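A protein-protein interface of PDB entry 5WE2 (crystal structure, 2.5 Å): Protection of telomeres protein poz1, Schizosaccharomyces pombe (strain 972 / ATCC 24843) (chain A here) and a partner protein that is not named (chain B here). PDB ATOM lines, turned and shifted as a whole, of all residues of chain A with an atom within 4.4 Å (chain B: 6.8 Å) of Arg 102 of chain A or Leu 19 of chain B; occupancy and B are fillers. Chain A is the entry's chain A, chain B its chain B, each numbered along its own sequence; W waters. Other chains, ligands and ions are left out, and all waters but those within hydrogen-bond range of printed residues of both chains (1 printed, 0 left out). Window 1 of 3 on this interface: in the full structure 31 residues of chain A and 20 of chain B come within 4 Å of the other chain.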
ATOM      1  N   LEU A  38       8.531   6.612  -8.329  1.00  0.00           N
ATOM      2  CA  LEU A  38       9.265   7.299  -9.377  1.00  0.00           C
ATOM      3  C   LEU A  38       9.462   6.333 -10.534  1.00  0.00           C
ATOM      4  O   LEU A  38       9.366   6.733 -11.677  1.00  0.00           O
ATOM      5  CB  LEU A  38      10.616   7.843  -8.862  1.00  0.00           C
ATOM      6  CG  LEU A  38      10.578   9.042  -7.902  1.00  0.00           C
ATOM      7  CD1 LEU A  38      11.950   9.274  -7.242  1.00  0.00           C
ATOM      8  CD2 LEU A  38      10.071  10.319  -8.594  1.00  0.00           C
ATOM      9  N   MET A  52       5.429  17.645 -16.262  1.00  0.00           N
ATOM     10  CA  MET A  52       5.912  17.425 -14.912  1.00  0.00           C
ATOM     11  C   MET A  52       5.262  18.455 -13.953  1.00  0.00           C
ATOM     12  O   MET A  52       5.427  19.667 -14.134  1.00  0.00           O
ATOM     13  CB  MET A  52       7.437  17.520 -14.896  1.00  0.00           C
ATOM     14  CG  MET A  52       8.035  17.304 -13.545  1.00  0.00           C
ATOM     15  SD  MET A  52       7.849  15.605 -12.992  1.00  0.00           S
ATOM     16  CE  MET A  52       8.875  14.766 -14.213  1.00  0.00           C
ATOM     17  N   ASP A  57       9.446  19.193  -9.800  1.00  0.00           N
ATOM     18  CA  ASP A  57      10.632  19.899 -10.234  1.00  0.00           C
ATOM     19  C   ASP A  57      11.261  20.524  -9.013  1.00  0.00           C
ATOM     20  O   ASP A  57      12.459  20.430  -8.813  1.00  0.00           O
ATOM     21  CB  ASP A  57      10.300  20.929 -11.314  1.00  0.00           C
ATOM     22  CG  ASP A  57      10.044  20.256 -12.698  1.00  0.00           C
ATOM     23  OD1 ASP A  57      10.626  19.187 -12.920  1.00  0.00           O
ATOM     24  OD2 ASP A  57       9.266  20.763 -13.536  1.00  0.00           O
ATOM     25  N   PHE A  60      12.859  18.057  -6.825  1.00  0.00           N
ATOM     26  CA  PHE A  60      14.074  17.593  -7.458  1.00  0.00           C
ATOM     27  C   PHE A  60      15.209  18.579  -7.220  1.00  0.00           C
ATOM     28  O   PHE A  60      16.307  18.183  -6.849  1.00  0.00           O
ATOM     29  CB  PHE A  60      13.902  17.348  -8.974  1.00  0.00           C
ATOM     30  CG  PHE A  60      15.212  17.095  -9.657  1.00  0.00           C
ATOM     31  CD1 PHE A  60      15.752  15.827  -9.666  1.00  0.00           C
ATOM     32  CD2 PHE A  60      15.941  18.145 -10.210  1.00  0.00           C
ATOM     33  CE1 PHE A  60      16.982  15.582 -10.242  1.00  0.00           C
ATOM     34  CE2 PHE A  60      17.153  17.923 -10.774  1.00  0.00           C
ATOM     35  CZ  PHE A  60      17.688  16.627 -10.809  1.00  0.00           C
ATOM     36  N   ASN A  98      19.981  18.926 -17.002  1.00  0.00           N
ATOM     37  CA  ASN A  98      18.563  18.661 -16.696  1.00  0.00           C
ATOM     38  C   ASN A  98      18.015  19.445 -15.495  1.00  0.00           C
ATOM     39  O   ASN A  98      16.841  19.848 -15.497  1.00  0.00           O
ATOM     40  CB  ASN A  98      18.318  17.166 -16.432  1.00  0.00           C
ATOM     41  CG  ASN A  98      18.611  16.332 -17.615  1.00  0.00           C
ATOM     42  OD1 ASN A  98      18.659  16.841 -18.728  1.00  0.00           O
ATOM     43  ND2 ASN A  98      18.819  15.026 -17.400  1.00  0.00           N
ATOM     44  N   ALA A  99      18.847  19.602 -14.453  1.00  0.00           N
ATOM     45  CA  ALA A  99      18.475  20.422 -13.290  1.00  0.00           C
ATOM     46  C   ALA A  99      18.180  21.842 -13.741  1.00  0.00           C
ATOM     47  O   ALA A  99      17.135  22.364 -13.421  1.00  0.00           O
ATOM     48  CB  ALA A  99      19.568  20.410 -12.212  1.00  0.00           C
ATOM     49  N   LEU A 100      19.066  22.444 -14.533  1.00  0.00           N
ATOM     50  CA  LEU A 100      18.828  23.818 -15.001  1.00  0.00           C
ATOM     51  C   LEU A 100      17.562  23.875 -15.839  1.00  0.00           C
ATOM     52  O   LEU A 100      16.818  24.860 -15.790  1.00  0.00           O
ATOM     53  CB  LEU A 100      20.020  24.359 -15.782  1.00  0.00           C
ATOM     54  CG  LEU A 100      21.183  24.786 -14.886  1.00  0.00           C
ATOM     55  CD1 LEU A 100      22.488  24.896 -15.657  1.00  0.00           C
ATOM     56  CD2 LEU A 100      20.866  26.103 -14.180  1.00  0.00           C
ATOM     57  N   GLU A 101      17.267  22.790 -16.557  1.00  0.00           N
ATOM     58  CA  GLU A 101      15.994  22.735 -17.277  1.00  0.00           C
ATOM     59  C   GLU A 101      14.791  22.758 -16.329  1.00  0.00           C
ATOM     60  O   GLU A 101      13.859  23.565 -16.492  1.00  0.00           O
ATOM     61  CB  GLU A 101      15.961  21.498 -18.157  1.00  0.00           C
ATOM     62  CG  GLU A 101      15.420  21.722 -19.552  1.00  0.00           C
ATOM     63  CD  GLU A 101      15.551  20.487 -20.439  1.00  0.00           C
ATOM     64  OE1 GLU A 101      16.683  20.171 -20.927  1.00  0.00           O
ATOM     65  OE2 GLU A 101      14.509  19.828 -20.631  1.00  0.00           O
ATOM     66  N   ARG A 102      14.808  21.889 -15.328  1.00  0.00           N
ATOM     67  CA  ARG A 102      13.722  21.842 -14.348  1.00  0.00           C
ATOM     68  C   ARG A 102      13.568  23.167 -13.574  1.00  0.00           C
ATOM     69  O   ARG A 102      12.447  23.576 -13.234  1.00  0.00           O
ATOM     70  CB  ARG A 102      13.943  20.690 -13.366  1.00  0.00           C
ATOM     71  CG  ARG A 102      13.887  19.317 -13.998  1.00  0.00           C
ATOM     72  CD  ARG A 102      14.137  18.200 -12.983  1.00  0.00           C
ATOM     73  NE  ARG A 102      14.233  16.904 -13.652  1.00  0.00           N
ATOM     74  CZ  ARG A 102      15.369  16.297 -14.000  1.00  0.00           C
ATOM     75  NH1 ARG A 102      16.545  16.832 -13.722  1.00  0.00           N
ATOM     76  NH2 ARG A 102      15.323  15.129 -14.628  1.00  0.00           N
ATOM     77  N   LEU A 103      14.688  23.839 -13.310  1.00  0.00           N
ATOM     78  CA  LEU A 103      14.667  25.140 -12.607  1.00  0.00           C
ATOM     79  C   LEU A 103      14.067  26.234 -13.485  1.00  0.00           C
ATOM     80  O   LEU A 103      13.347  27.131 -13.000  1.00  0.00           O
ATOM     81  CB  LEU A 103      16.075  25.573 -12.150  1.00  0.00           C
ATOM     82  CG  LEU A 103      16.247  26.885 -11.343  1.00  0.00           C
ATOM     83  CD1 LEU A 103      15.676  26.836  -9.899  1.00  0.00           C
ATOM     84  CD2 LEU A 103      17.718  27.332 -11.278  1.00  0.00           C
ATOM     85  N   GLU A 104      14.392  26.160 -14.772  1.00  0.00           N
ATOM     86  CA  GLU A 104      13.854  27.080 -15.769  1.00  0.00           C
ATOM     87  C   GLU A 104      12.348  26.922 -15.834  1.00  0.00           C
ATOM     88  O   GLU A 104      11.607  27.906 -15.826  1.00  0.00           O
ATOM     89  CB  GLU A 104      14.509  26.809 -17.134  1.00  0.00           C
ATOM     90  CG  GLU A 104      14.073  27.715 -18.303  1.00  0.00           C
ATOM     91  CD  GLU A 104      14.876  27.445 -19.580  1.00  0.00           C
ATOM     92  OE1 GLU A 104      14.670  26.373 -20.213  1.00  0.00           O
ATOM     93  OE2 GLU A 104      15.715  28.304 -19.958  1.00  0.00           O
ATOM     94  N   ASN A 105      11.906  25.668 -15.884  1.00  0.00           N
ATOM     95  CA  ASN A 105      10.490  25.332 -15.804  1.00  0.00           C
ATOM     96  C   ASN A 105       9.823  25.866 -14.548  1.00  0.00           C
ATOM     97  O   ASN A 105       8.661  26.305 -14.576  1.00  0.00           O
ATOM     98  CB  ASN A 105      10.299  23.807 -15.856  1.00  0.00           C
ATOM     99  CG  ASN A 105      10.622  23.224 -17.220  1.00  0.00           C
ATOM    100  OD1 ASN A 105      11.009  23.945 -18.152  1.00  0.00           O
ATOM    101  ND2 ASN A 105      10.516  21.899 -17.331  1.00  0.00           N
ATOM    102  N   ILE A 106      10.523  25.768 -13.423  1.00  0.00           N
ATOM    103  CA  ILE A 106       9.966  26.336 -12.193  1.00  0.00           C
ATOM    104  C   ILE A 106       9.752  27.833 -12.389  1.00  0.00           C
ATOM    105  O   ILE A 106       8.662  28.343 -12.169  1.00  0.00           O
ATOM    106  CB  ILE A 106      10.865  26.078 -10.985  1.00  0.00           C
ATOM    107  CG1 ILE A 106      10.909  24.574 -10.693  1.00  0.00           C
ATOM    108  CG2 ILE A 106      10.367  26.861  -9.751  1.00  0.00           C
ATOM    109  CD1 ILE A 106      11.985  24.202  -9.642  1.00  0.00           C
ATOM    110  N   GLY B  14      10.848  10.545 -22.013  1.00  0.00           N
ATOM    111  CA  GLY B  14      10.050  11.626 -21.446  1.00  0.00           C
ATOM    112  C   GLY B  14      10.453  12.052 -20.040  1.00  0.00           C
ATOM    113  O   GLY B  14      11.393  11.498 -19.457  1.00  0.00           O
ATOM    114  N   SER B  15       9.706  13.001 -19.476  1.00  0.00           N
ATOM    115  CA  SER B  15      10.232  13.786 -18.377  1.00  0.00           C
ATOM    116  C   SER B  15      10.215  12.995 -17.072  1.00  0.00           C
ATOM    117  O   SER B  15      11.135  13.105 -16.270  1.00  0.00           O
ATOM    118  CB  SER B  15       9.476  15.116 -18.248  1.00  0.00           C
ATOM    119  OG  SER B  15       8.321  14.993 -17.448  1.00  0.00           O
ATOM    120  N   PHE B  16       9.210  12.156 -16.883  1.00  0.00           N
ATOM    121  CA  PHE B  16       9.194  11.261 -15.736  1.00  0.00           C
ATOM    122  C   PHE B  16      10.314  10.232 -15.777  1.00  0.00           C
ATOM    123  O   PHE B  16      10.941   9.936 -14.741  1.00  0.00           O
ATOM    124  CB  PHE B  16       7.845  10.579 -15.639  1.00  0.00           C
ATOM    125  CG  PHE B  16       6.742  11.524 -15.314  1.00  0.00           C
ATOM    126  CD1 PHE B  16       6.534  11.944 -14.000  1.00  0.00           C
ATOM    127  CD2 PHE B  16       5.952  12.053 -16.313  1.00  0.00           C
ATOM    128  CE1 PHE B  16       5.506  12.847 -13.679  1.00  0.00           C
ATOM    129  CE2 PHE B  16       4.932  12.961 -16.006  1.00  0.00           C
ATOM    130  CZ  PHE B  16       4.717  13.363 -14.671  1.00  0.00           C
ATOM    131  N   PHE B  17      10.599   9.710 -16.969  1.00  0.00           N
ATOM    132  CA  PHE B  17      11.696   8.772 -17.109  1.00  0.00           C
ATOM    133  C   PHE B  17      13.040   9.455 -16.866  1.00  0.00           C
ATOM    134  O   PHE B  17      13.913   8.927 -16.142  1.00  0.00           O
ATOM    135  CB  PHE B  17      11.648   8.101 -18.506  1.00  0.00           C
ATOM    136  CG  PHE B  17      12.815   7.196 -18.783  1.00  0.00           C
ATOM    137  CD1 PHE B  17      13.006   6.043 -18.033  1.00  0.00           C
ATOM    138  CD2 PHE B  17      13.737   7.514 -19.781  1.00  0.00           C
ATOM    139  CE1 PHE B  17      14.100   5.199 -18.282  1.00  0.00           C
ATOM    140  CE2 PHE B  17      14.826   6.679 -20.040  1.00  0.00           C
ATOM    141  CZ  PHE B  17      15.007   5.515 -19.291  1.00  0.00           C
ATOM    142  N   GLU B  18      13.213  10.639 -17.448  1.00  0.00           N
ATOM    143  CA  GLU B  18      14.431  11.419 -17.195  1.00  0.00           C
ATOM    144  C   GLU B  18      14.624  11.741 -15.687  1.00  0.00           C
ATOM    145  O   GLU B  18      15.719  11.614 -15.145  1.00  0.00           O
ATOM    146  CB  GLU B  18      14.412  12.707 -18.013  1.00  0.00           C
ATOM    147  CG  GLU B  18      14.511  12.538 -19.515  1.00  0.00           C
ATOM    148  CD  GLU B  18      15.628  11.579 -19.935  1.00  0.00           C
ATOM    149  OE1 GLU B  18      16.707  11.593 -19.295  1.00  0.00           O
ATOM    150  OE2 GLU B  18      15.421  10.796 -20.907  1.00  0.00           O
ATOM    151  N   LEU B  19      13.536  12.102 -15.013  1.00  0.00           N
ATOM    152  CA  LEU B  19      13.545  12.368 -13.581  1.00  0.00           C
ATOM    153  C   LEU B  19      13.966  11.133 -12.799  1.00  0.00           C
ATOM    154  O   LEU B  19      14.794  11.211 -11.870  1.00  0.00           O
ATOM    155  CB  LEU B  19      12.159  12.836 -13.106  1.00  0.00           C
ATOM    156  CG  LEU B  19      12.054  13.033 -11.587  1.00  0.00           C
ATOM    157  CD1 LEU B  19      12.881  14.246 -11.251  1.00  0.00           C
ATOM    158  CD2 LEU B  19      10.626  13.209 -11.148  1.00  0.00           C
ATOM    159  N   LEU B  20      13.403   9.989 -13.175  1.00  0.00           N
ATOM    160  CA  LEU B  20      13.792   8.728 -12.548  1.00  0.00           C
ATOM    161  C   LEU B  20      15.300   8.473 -12.629  1.00  0.00           C
ATOM    162  O   LEU B  20      15.968   8.108 -11.632  1.00  0.00           O
ATOM    163  CB  LEU B  20      13.040   7.578 -13.203  1.00  0.00           C
ATOM    164  CG  LEU B  20      13.494   6.175 -12.822  1.00  0.00           C
ATOM    165  CD1 LEU B  20      13.067   5.894 -11.378  1.00  0.00           C
ATOM    166  CD2 LEU B  20      12.967   5.117 -13.850  1.00  0.00           C
ATOM    167  N   ARG B  21      15.854   8.670 -13.818  1.00  0.00           N
ATOM    168  CA  ARG B  21      17.276   8.353 -13.985  1.00  0.00           C
ATOM    169  C   ARG B  21      18.194   9.313 -13.226  1.00  0.00           C
ATOM    170  O   ARG B  21      19.188   8.895 -12.612  1.00  0.00           O
ATOM    171  CB  ARG B  21      17.644   8.347 -15.466  1.00  0.00           C
ATOM    172  CG  ARG B  21      17.085   7.154 -16.194  1.00  0.00           C
ATOM    173  CD  ARG B  21      17.950   6.808 -17.370  1.00  0.00           C
ATOM    174  NE  ARG B  21      17.998   7.934 -18.288  1.00  0.00           N
ATOM    175  CZ  ARG B  21      18.440   7.877 -19.541  1.00  0.00           C
ATOM    176  NH1 ARG B  21      18.874   6.725 -20.063  1.00  0.00           N
ATOM    177  NH2 ARG B  21      18.432   8.986 -20.272  1.00  0.00           N
ATOM    178  N   ASP B  22      17.863  10.601 -13.287  1.00  0.00           N
ATOM    179  CA  ASP B  22      18.617  11.611 -12.545  1.00  0.00           C
ATOM    180  C   ASP B  22      18.541  11.377 -11.027  1.00  0.00           C
ATOM    181  O   ASP B  22      19.548  11.391 -10.319  1.00  0.00           O
ATOM    182  CB  ASP B  22      18.099  12.988 -12.920  1.00  0.00           C
ATOM    183  CG  ASP B  22      18.542  13.403 -14.321  1.00  0.00           C
ATOM    184  OD1 ASP B  22      19.431  12.695 -14.888  1.00  0.00           O
ATOM    185  OD2 ASP B  22      18.027  14.434 -14.837  1.00  0.00           O
ATOM    186  N   TRP B  23      17.340  11.092 -10.554  1.00  0.00           N
ATOM    187  CA  TRP B  23      17.118  10.727  -9.164  1.00  0.00           C
ATOM    188  C   TRP B  23      18.013   9.582  -8.694  1.00  0.00           C
ATOM    189  O   TRP B  23      18.663   9.682  -7.624  1.00  0.00           O
ATOM    190  CB  TRP B  23      15.656  10.351  -8.956  1.00  0.00           C
ATOM    191  CG  TRP B  23      15.238  10.480  -7.546  1.00  0.00           C
ATOM    192  CD1 TRP B  23      15.476   9.599  -6.527  1.00  0.00           C
ATOM    193  CD2 TRP B  23      14.524  11.575  -6.975  1.00  0.00           C
ATOM    194  NE1 TRP B  23      14.928  10.070  -5.360  1.00  0.00           N
ATOM    195  CE2 TRP B  23      14.342  11.287  -5.609  1.00  0.00           C
ATOM    196  CE3 TRP B  23      14.000  12.759  -7.493  1.00  0.00           C
ATOM    197  CZ2 TRP B  23      13.669  12.155  -4.749  1.00  0.00           C
ATOM    198  CZ3 TRP B  23      13.327  13.617  -6.637  1.00  0.00           C
ATOM    199  CH2 TRP B  23      13.172  13.315  -5.285  1.00  0.00           C
ATOM    200  N   LYS B  24      18.063   8.502  -9.482  1.00  0.00           N
ATOM    201  CA  LYS B  24      18.969   7.373  -9.169  1.00  0.00           C
ATOM    202  C   LYS B  24      20.464   7.722  -9.220  1.00  0.00           C
ATOM    203  O   LYS B  24      21.249   7.234  -8.411  1.00  0.00           O
ATOM    204  CB  LYS B  24      18.690   6.196 -10.119  1.00  0.00           C
ATOM    205  CG  LYS B  24      17.193   5.792 -10.152  1.00  0.00           C
ATOM    206  CD  LYS B  24      17.003   4.306 -10.364  1.00  0.00           C
ATOM    207  CE  LYS B  24      17.752   3.794 -11.603  1.00  0.00           C
ATOM    208  NZ  LYS B  24      18.244   2.397 -11.383  1.00  0.00           N
HETATM  209  O   HOH W   1       9.510   9.680 -12.405  1.00  0.00           O
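The side-chain amide nitrogen of Asn 98 of chain A sits at hydrogen-bond distance from the side-chain carboxylate of Asp 22 of chain B (2.7 Å).
The guanidinium group (NH2) of Arg 102 of chain A is in salt-bridge range of the side-chain carboxylate (OD2) of Asp 22 of chain B, at 2.8 Å.
The side-chain carboxylate of Glu 18 of chain B lies within salt-bridge range of the guanidinium group of Arg 21 of chain B.
CD2 of Leu 19 of chain B touches CD2 of Leu 38 of chain A, at 3.9 Å.
C of Leu 38 of chain A touches CD1 of Leu 20 of chain B, 3.7 Å away.
Trp 23 of chain B touches Leu 38 of chain A.
Ser 15 of chain B touches Met 52 of chain A.
Met 52 of chain A touches Phe 16 of chain B.
Met 52 of chain A touches Leu 19 of chain B (CE to CD2, 3.9 Å).
CD1 of Leu 19 of chain B touches CD1 of Phe 60 of chain A, at 3.6 Å.
Asp 22 of chain B touches Phe 60 of chain A (CB to CE1, 3.9 Å).
Glu 18 of chain B touches Arg 102 of chain A (O to NH2, 3.6 Å).
Leu 19 of chain B touches Arg 102 of chain A (CA to NH2, 3.4 Å).
Printed residues of chain B within 4 Å of Leu 38 of chain A: Leu 19 (3.9 Å), Leu 20 (3.7 Å) and Trp 23 (3.5 Å).
Of the printed residues of chain B, Asn 98 of chain A touches Asp 22.
Glu 101 of chain A touches none of the printed residues of chain B.
Of the printed residues of chain A, Phe 16 of chain B touches Met 52 (3.7 Å).
Printed residues of chain A within 4 Å of Glu 18 of chain B: Arg 102.
Of the printed residues of chain A, Leu 19 of chain B touches Leu 38 (3.9 Å), Met 52 (3.9 Å), Phe 60 (3.6 Å) and Arg 102 (3.4 Å).
Printed residues of chain A within 4 Å of Trp 23 of chain B: Leu 38.
Lys 24 of chain B touches none of the printed residues of chain A.
The nearest printed residue of chain A that does not touch Leu 19 of chain B is Asp 57 of chain A (5.7 Å).
The nearest printed residue of chain B that does not touch Leu 38 of chain A is Phe 16 of chain B (4.7 Å).
Of the 13 printed residues of chain A, 5 touch a printed residue of chain B.
Printed residues of chain A that touch a printed residue of chain B: Leu 38, Met 52, Phe 60, Asn 98 and Arg 102.
Of the 11 printed residues of chain B, 7 touch a printed residue of chain A.
Printed residues of chain B that touch a printed residue of chain A: Ser 15, Phe 16, Glu 18, Leu 19, Leu 20, Asp 22 and Trp 23.
Hydrophobic or aromatic side chains of chain B that line the printed part of chain A: Phe 16, Leu 19, Leu 20 and Trp 23.
Among the printed residues, 12 pairs touch across the chains.
Among the printed residues, Asp or Glu carboxylates within 4 Å of a Lys or Arg side-chain nitrogen of the other chain: Arg 102 of chain A with Asp 22 of chain B (2.8 Å).
Water W1 bridges O of Phe 16 of chain B (2.8 Å) and O of Leu 38 of chain A (3.0 Å).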
